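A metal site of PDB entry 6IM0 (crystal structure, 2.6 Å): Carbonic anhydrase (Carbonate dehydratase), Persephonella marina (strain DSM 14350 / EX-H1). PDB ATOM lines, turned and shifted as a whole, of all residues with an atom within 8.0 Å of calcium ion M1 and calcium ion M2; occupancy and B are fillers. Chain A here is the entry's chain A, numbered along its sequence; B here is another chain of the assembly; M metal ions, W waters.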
ATOM      1  N   ILE A  58     -25.524  26.880 -23.209  1.00  0.00           N
ATOM      2  CA  ILE A  58     -24.814  27.190 -21.999  1.00  0.00           C
ATOM      3  C   ILE A  58     -23.599  26.278 -21.911  1.00  0.00           C
ATOM      4  O   ILE A  58     -23.685  25.083 -22.165  1.00  0.00           O
ATOM      5  CB  ILE A  58     -25.712  26.957 -20.774  1.00  0.00           C
ATOM      6  CG1 ILE A  58     -26.994  27.765 -20.907  1.00  0.00           C
ATOM      7  CG2 ILE A  58     -24.975  27.332 -19.499  1.00  0.00           C
ATOM      8  CD1 ILE A  58     -28.095  27.411 -19.900  1.00  0.00           C
ATOM      9  N   VAL A  59     -22.487  26.836 -21.481  1.00  0.00           N
ATOM     10  CA  VAL A  59     -21.342  26.020 -21.241  1.00  0.00           C
ATOM     11  C   VAL A  59     -20.754  26.366 -19.895  1.00  0.00           C
ATOM     12  O   VAL A  59     -20.579  27.530 -19.571  1.00  0.00           O
ATOM     13  CB  VAL A  59     -20.349  26.136 -22.402  1.00  0.00           C
ATOM     14  CG1 VAL A  59     -19.806  27.517 -22.503  1.00  0.00           C
ATOM     15  CG2 VAL A  59     -19.201  25.141 -22.258  1.00  0.00           C
ATOM     16  N   ASP A  60     -20.398  25.350 -19.126  1.00  0.00           N
ATOM     17  CA  ASP A  60     -19.702  25.552 -17.876  1.00  0.00           C
ATOM     18  C   ASP A  60     -18.368  26.223 -18.171  1.00  0.00           C
ATOM     19  O   ASP A  60     -17.662  25.850 -19.105  1.00  0.00           O
ATOM     20  CB  ASP A  60     -19.501  24.212 -17.151  1.00  0.00           C
ATOM     21  CG  ASP A  60     -20.803  23.515 -16.820  1.00  0.00           C
ATOM     22  OD1 ASP A  60     -21.789  24.187 -16.455  1.00  0.00           O
ATOM     23  OD2 ASP A  60     -20.851  22.281 -16.867  1.00  0.00           O
ATOM     24  N   ALA A  61     -18.025  27.213 -17.374  1.00  0.00           N
ATOM     25  CA  ALA A  61     -16.751  27.900 -17.486  1.00  0.00           C
ATOM     26  C   ALA A  61     -16.229  28.369 -16.129  1.00  0.00           C
ATOM     27  O   ALA A  61     -17.003  28.721 -15.271  1.00  0.00           O
ATOM     28  CB  ALA A  61     -16.906  29.078 -18.414  1.00  0.00           C
ATOM     29  N   LYS A 117     -33.621  29.003 -20.763  1.00  0.00           N
ATOM     30  CA  LYS A 117     -34.024  27.758 -21.421  1.00  0.00           C
ATOM     31  C   LYS A 117     -35.467  27.806 -21.908  1.00  0.00           C
ATOM     32  O   LYS A 117     -36.294  26.976 -21.552  1.00  0.00           O
ATOM     33  CB  LYS A 117     -33.720  26.546 -20.511  1.00  0.00           C
ATOM     34  CG  LYS A 117     -32.266  26.119 -20.635  1.00  0.00           C
ATOM     35  CD  LYS A 117     -31.861  24.963 -19.731  1.00  0.00           C
ATOM     36  CE  LYS A 117     -30.632  24.245 -20.258  1.00  0.00           C
ATOM     37  NZ  LYS A 117     -29.916  23.504 -19.172  1.00  0.00           N
ATOM     38  N   TYR A 186     -24.275  33.874 -15.209  1.00  0.00           N
ATOM     39  CA  TYR A 186     -24.091  33.680 -16.632  1.00  0.00           C
ATOM     40  C   TYR A 186     -23.401  34.901 -17.225  1.00  0.00           C
ATOM     41  O   TYR A 186     -23.706  36.031 -16.848  1.00  0.00           O
ATOM     42  CB  TYR A 186     -25.409  33.505 -17.359  1.00  0.00           C
ATOM     43  CG  TYR A 186     -26.230  32.353 -16.857  1.00  0.00           C
ATOM     44  CD1 TYR A 186     -25.871  31.037 -17.137  1.00  0.00           C
ATOM     45  CD2 TYR A 186     -27.397  32.566 -16.131  1.00  0.00           C
ATOM     46  CE1 TYR A 186     -26.627  29.975 -16.698  1.00  0.00           C
ATOM     47  CE2 TYR A 186     -28.175  31.514 -15.687  1.00  0.00           C
ATOM     48  CZ  TYR A 186     -27.778  30.220 -15.958  1.00  0.00           C
ATOM     49  OH  TYR A 186     -28.555  29.186 -15.478  1.00  0.00           O
ATOM     50  N   GLU A 207     -27.506  33.765 -11.688  1.00  0.00           N
ATOM     51  CA  GLU A 207     -28.269  32.498 -11.732  1.00  0.00           C
ATOM     52  C   GLU A 207     -29.375  32.443 -10.693  1.00  0.00           C
ATOM     53  O   GLU A 207     -30.435  31.934 -10.978  1.00  0.00           O
ATOM     54  CB  GLU A 207     -27.383  31.279 -11.509  1.00  0.00           C
ATOM     55  CG  GLU A 207     -26.263  31.139 -12.525  1.00  0.00           C
ATOM     56  CD  GLU A 207     -25.356  29.942 -12.268  1.00  0.00           C
ATOM     57  OE1 GLU A 207     -24.124  30.067 -12.491  1.00  0.00           O
ATOM     58  OE2 GLU A 207     -25.898  28.881 -11.848  1.00  0.00           O
ATOM     59  N   MET A 241     -21.700  31.529 -21.021  1.00  0.00           N
ATOM     60  CA  MET A 241     -20.886  30.914 -20.001  1.00  0.00           C
ATOM     61  C   MET A 241     -21.612  30.885 -18.655  1.00  0.00           C
ATOM     62  O   MET A 241     -22.217  31.882 -18.253  1.00  0.00           O
ATOM     63  CB  MET A 241     -19.601  31.681 -19.852  1.00  0.00           C
ATOM     64  CG  MET A 241     -18.732  31.655 -21.080  1.00  0.00           C
ATOM     65  SD  MET A 241     -17.782  33.184 -21.216  1.00  0.00           S
ATOM     66  CE  MET A 241     -16.258  32.369 -21.279  1.00  0.00           C
ATOM     67  N   GLU A 242     -21.479  29.764 -17.935  1.00  0.00           N
ATOM     68  CA  GLU A 242     -22.054  29.549 -16.595  1.00  0.00           C
ATOM     69  C   GLU A 242     -20.973  29.245 -15.556  1.00  0.00           C
ATOM     70  O   GLU A 242     -20.194  28.283 -15.704  1.00  0.00           O
ATOM     71  CB  GLU A 242     -23.016  28.370 -16.603  1.00  0.00           C
ATOM     72  CG  GLU A 242     -23.712  28.145 -15.258  1.00  0.00           C
ATOM     73  CD  GLU A 242     -24.460  26.830 -15.128  1.00  0.00           C
ATOM     74  OE1 GLU A 242     -24.803  26.185 -16.142  1.00  0.00           O
ATOM     75  OE2 GLU A 242     -24.722  26.418 -13.977  1.00  0.00           O
ATOM     76  N   LYS A 243     -20.939  30.027 -14.486  1.00  0.00           N
ATOM     77  CA  LYS A 243     -19.981  29.848 -13.413  1.00  0.00           C
ATOM     78  C   LYS A 243     -20.241  28.592 -12.539  1.00  0.00           C
ATOM     79  O   LYS A 243     -21.364  28.360 -12.074  1.00  0.00           O
ATOM     80  CB  LYS A 243     -19.963  31.100 -12.551  1.00  0.00           C
ATOM     81  CG  LYS A 243     -18.824  31.130 -11.560  1.00  0.00           C
ATOM     82  CD  LYS A 243     -18.783  32.409 -10.785  1.00  0.00           C
ATOM     83  CE  LYS A 243     -17.609  32.455  -9.820  1.00  0.00           C
ATOM     84  NZ  LYS A 243     -17.783  31.505  -8.692  1.00  0.00           N
ATOM     85  N   TYR B 121     -33.864  16.084 -18.964  1.00  0.00           N
ATOM     86  CA  TYR B 121     -32.499  15.868 -19.471  1.00  0.00           C
ATOM     87  C   TYR B 121     -32.521  14.506 -20.160  1.00  0.00           C
ATOM     88  O   TYR B 121     -33.403  13.686 -19.880  1.00  0.00           O
ATOM     89  CB  TYR B 121     -31.498  15.866 -18.338  1.00  0.00           C
ATOM     90  CG  TYR B 121     -31.181  17.229 -17.745  1.00  0.00           C
ATOM     91  CD1 TYR B 121     -32.005  17.769 -16.747  1.00  0.00           C
ATOM     92  CD2 TYR B 121     -30.053  17.939 -18.120  1.00  0.00           C
ATOM     93  CE1 TYR B 121     -31.688  18.987 -16.148  1.00  0.00           C
ATOM     94  CE2 TYR B 121     -29.762  19.162 -17.553  1.00  0.00           C
ATOM     95  CZ  TYR B 121     -30.573  19.677 -16.572  1.00  0.00           C
ATOM     96  OH  TYR B 121     -30.302  20.903 -15.994  1.00  0.00           O
ATOM     97  N   PHE B 142     -28.244  14.834 -13.072  1.00  0.00           N
ATOM     98  CA  PHE B 142     -28.642  14.978 -14.464  1.00  0.00           C
ATOM     99  C   PHE B 142     -27.403  14.944 -15.356  1.00  0.00           C
ATOM    100  O   PHE B 142     -26.369  15.472 -15.009  1.00  0.00           O
ATOM    101  CB  PHE B 142     -29.351  16.320 -14.708  1.00  0.00           C
ATOM    102  CG  PHE B 142     -30.664  16.459 -14.027  1.00  0.00           C
ATOM    103  CD1 PHE B 142     -31.704  15.576 -14.293  1.00  0.00           C
ATOM    104  CD2 PHE B 142     -30.897  17.513 -13.122  1.00  0.00           C
ATOM    105  CE1 PHE B 142     -32.946  15.733 -13.666  1.00  0.00           C
ATOM    106  CE2 PHE B 142     -32.110  17.676 -12.499  1.00  0.00           C
ATOM    107  CZ  PHE B 142     -33.150  16.787 -12.772  1.00  0.00           C
ATOM    108  N   LYS B 144     -26.362  15.939 -19.465  1.00  0.00           N
ATOM    109  CA  LYS B 144     -26.695  16.433 -20.826  1.00  0.00           C
ATOM    110  C   LYS B 144     -25.719  15.864 -21.886  1.00  0.00           C
ATOM    111  O   LYS B 144     -24.683  15.306 -21.528  1.00  0.00           O
ATOM    112  CB  LYS B 144     -26.659  17.962 -20.861  1.00  0.00           C
ATOM    113  CG  LYS B 144     -25.298  18.597 -20.595  1.00  0.00           C
ATOM    114  CD  LYS B 144     -25.288  20.063 -21.038  1.00  0.00           C
ATOM    115  CE  LYS B 144     -23.983  20.749 -20.660  1.00  0.00           C
ATOM    116  NZ  LYS B 144     -23.943  22.183 -21.089  1.00  0.00           N
ATOM    117  N   PRO B 180     -20.906  16.492  -9.625  1.00  0.00           N
ATOM    118  CA  PRO B 180     -20.362  17.794  -9.896  1.00  0.00           C
ATOM    119  C   PRO B 180     -19.546  18.347  -8.746  1.00  0.00           C
ATOM    120  O   PRO B 180     -19.638  17.835  -7.635  1.00  0.00           O
ATOM    121  CB  PRO B 180     -21.609  18.642 -10.154  1.00  0.00           C
ATOM    122  CG  PRO B 180     -22.705  17.960  -9.447  1.00  0.00           C
ATOM    123  CD  PRO B 180     -22.383  16.505  -9.542  1.00  0.00           C
ATOM    124  N   LYS B 181     -18.748  19.361  -9.038  1.00  0.00           N
ATOM    125  CA  LYS B 181     -17.960  20.087  -8.039  1.00  0.00           C
ATOM    126  C   LYS B 181     -18.777  21.169  -7.348  1.00  0.00           C
ATOM    127  O   LYS B 181     -18.598  21.371  -6.182  1.00  0.00           O
ATOM    128  CB  LYS B 181     -16.692  20.688  -8.671  1.00  0.00           C
ATOM    129  CG  LYS B 181     -15.505  19.738  -8.616  1.00  0.00           C
ATOM    130  CD  LYS B 181     -14.610  19.770  -9.867  1.00  0.00           C
ATOM    131  CE  LYS B 181     -13.270  19.051  -9.637  1.00  0.00           C
ATOM    132  NZ  LYS B 181     -13.391  17.655  -9.072  1.00  0.00           N
ATOM    133  N   ASP B 182     -19.682  21.828  -8.079  1.00  0.00           N
ATOM    134  CA  ASP B 182     -20.786  22.637  -7.480  1.00  0.00           C
ATOM    135  C   ASP B 182     -21.747  21.598  -6.857  1.00  0.00           C
ATOM    136  O   ASP B 182     -22.352  20.788  -7.566  1.00  0.00           O
ATOM    137  CB  ASP B 182     -21.532  23.537  -8.546  1.00  0.00           C
ATOM    138  CG  ASP B 182     -22.439  24.670  -7.903  1.00  0.00           C
ATOM    139  OD1 ASP B 182     -22.448  24.835  -6.659  1.00  0.00           O
ATOM    140  OD2 ASP B 182     -23.147  25.419  -8.638  1.00  0.00           O
ATOM    141  N   GLU B 207     -28.051  20.366  -8.614  1.00  0.00           N
ATOM    142  CA  GLU B 207     -28.453  21.432  -9.560  1.00  0.00           C
ATOM    143  C   GLU B 207     -27.609  21.422 -10.790  1.00  0.00           C
ATOM    144  O   GLU B 207     -28.090  21.682 -11.876  1.00  0.00           O
ATOM    145  CB  GLU B 207     -28.395  22.821  -8.933  1.00  0.00           C
ATOM    146  CG  GLU B 207     -29.312  23.014  -7.731  1.00  0.00           C
ATOM    147  CD  GLU B 207     -29.213  24.404  -7.103  1.00  0.00           C
ATOM    148  OE1 GLU B 207     -29.283  24.489  -5.832  1.00  0.00           O
ATOM    149  OE2 GLU B 207     -29.078  25.400  -7.864  1.00  0.00           O
ATOM    150  N   GLU B 208     -26.320  21.148 -10.628  1.00  0.00           N
ATOM    151  CA  GLU B 208     -25.415  21.171 -11.752  1.00  0.00           C
ATOM    152  C   GLU B 208     -25.408  19.815 -12.445  1.00  0.00           C
ATOM    153  O   GLU B 208     -25.212  18.772 -11.817  1.00  0.00           O
ATOM    154  CB  GLU B 208     -24.000  21.607 -11.326  1.00  0.00           C
ATOM    155  CG  GLU B 208     -22.940  21.637 -12.438  1.00  0.00           C
ATOM    156  CD  GLU B 208     -23.286  22.524 -13.610  1.00  0.00           C
ATOM    157  OE1 GLU B 208     -24.051  23.512 -13.470  1.00  0.00           O
ATOM    158  OE2 GLU B 208     -22.769  22.251 -14.703  1.00  0.00           O
ATOM    159  N   GLU B 209     -25.631  19.870 -13.754  1.00  0.00           N
ATOM    160  CA  GLU B 209     -25.622  18.694 -14.603  1.00  0.00           C
ATOM    161  C   GLU B 209     -24.188  18.267 -14.938  1.00  0.00           C
ATOM    162  O   GLU B 209     -23.263  19.091 -14.916  1.00  0.00           O
ATOM    163  CB  GLU B 209     -26.398  18.980 -15.906  1.00  0.00           C
ATOM    164  CG  GLU B 209     -25.633  19.720 -17.031  1.00  0.00           C
ATOM    165  CD  GLU B 209     -25.063  21.070 -16.630  1.00  0.00           C
ATOM    166  OE1 GLU B 209     -25.810  21.867 -16.009  1.00  0.00           O
ATOM    167  OE2 GLU B 209     -23.878  21.339 -16.966  1.00  0.00           O
ATOM    168  N   MET B 210     -24.064  17.027 -15.371  1.00  0.00           N
ATOM    169  CA  MET B 210     -22.812  16.470 -15.864  1.00  0.00           C
ATOM    170  C   MET B 210     -23.001  16.199 -17.341  1.00  0.00           C
ATOM    171  O   MET B 210     -24.093  16.420 -17.859  1.00  0.00           O
ATOM    172  CB  MET B 210     -22.487  15.189 -15.120  1.00  0.00           C
ATOM    173  CG  MET B 210     -22.163  15.401 -13.653  1.00  0.00           C
ATOM    174  SD  MET B 210     -20.724  16.426 -13.285  1.00  0.00           S
ATOM    175  CE  MET B 210     -19.417  15.219 -13.414  1.00  0.00           C
ATOM    176  N   GLU B 211     -21.937  15.735 -18.000  1.00  0.00           N
ATOM    177  CA  GLU B 211     -21.927  15.522 -19.440  1.00  0.00           C
ATOM    178  C   GLU B 211     -21.678  14.077 -19.811  1.00  0.00           C
ATOM    179  O   GLU B 211     -20.972  13.341 -19.139  1.00  0.00           O
ATOM    180  CB  GLU B 211     -20.840  16.335 -20.089  1.00  0.00           C
ATOM    181  CG  GLU B 211     -21.123  17.820 -20.256  1.00  0.00           C
ATOM    182  CD  GLU B 211     -20.073  18.507 -21.128  1.00  0.00           C
ATOM    183  OE1 GLU B 211     -18.875  18.210 -20.911  1.00  0.00           O
ATOM    184  OE2 GLU B 211     -20.437  19.330 -22.022  1.00  0.00           O
HETATM  185 CA    CA M   1     -24.147  23.759 -16.115  1.00  0.00          CA
HETATM  186 CA    CA M   2     -21.499  20.568 -15.771  1.00  0.00          CA
HETATM  187  O   HOH W   1     -20.407  18.773 -17.369  1.00  0.00           O
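Of the 21 residues printed, 3 come within 4 Å of calcium ion M2.
The nearest printed residue that does not touch calcium ion M2 is Met 210 of chain B (4.3 Å).
The backbone carbonyl oxygen (O) of Glu 242 is in hydrogen-bond range of the backbone NH (N) of Ala 61, at 2.9 Å.
The backbone carbonyl oxygen of Val 59 lies within hydrogen-bond range of the backbone NH of Glu 242.
Calcium ion M1 is bound by the side-chain carboxylate (OD1) of Asp 60 (2.4 Å), the side-chain carboxylate (OE2) of Glu 208 of chain B (2.5 Å), the side-chain carboxylate (OE1) of Glu 242 (2.5 Å), the side-chain carboxylate (OE1) of Glu 209 of chain B (2.5 Å), the side-chain carboxylate (OE2) of Glu 209 of chain B (2.6 Å) and the side-chain carboxylate (OE1) of Glu 208 of chain B (2.7 Å).
Calcium ion M2 is bound by the side-chain carboxylate of Asp 60 (2.1 Å), the side-chain carboxylate of Glu 208 of chain B (2.4 Å), the backbone carbonyl oxygen of Glu 209 of chain B (2.5 Å), water W1 (2.6 Å) and the side-chain carboxylate of Glu 209 of chain B (2.8 Å).
The nearest printed residue that does not touch calcium ion M1 is Ile 58 (5.0 Å).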
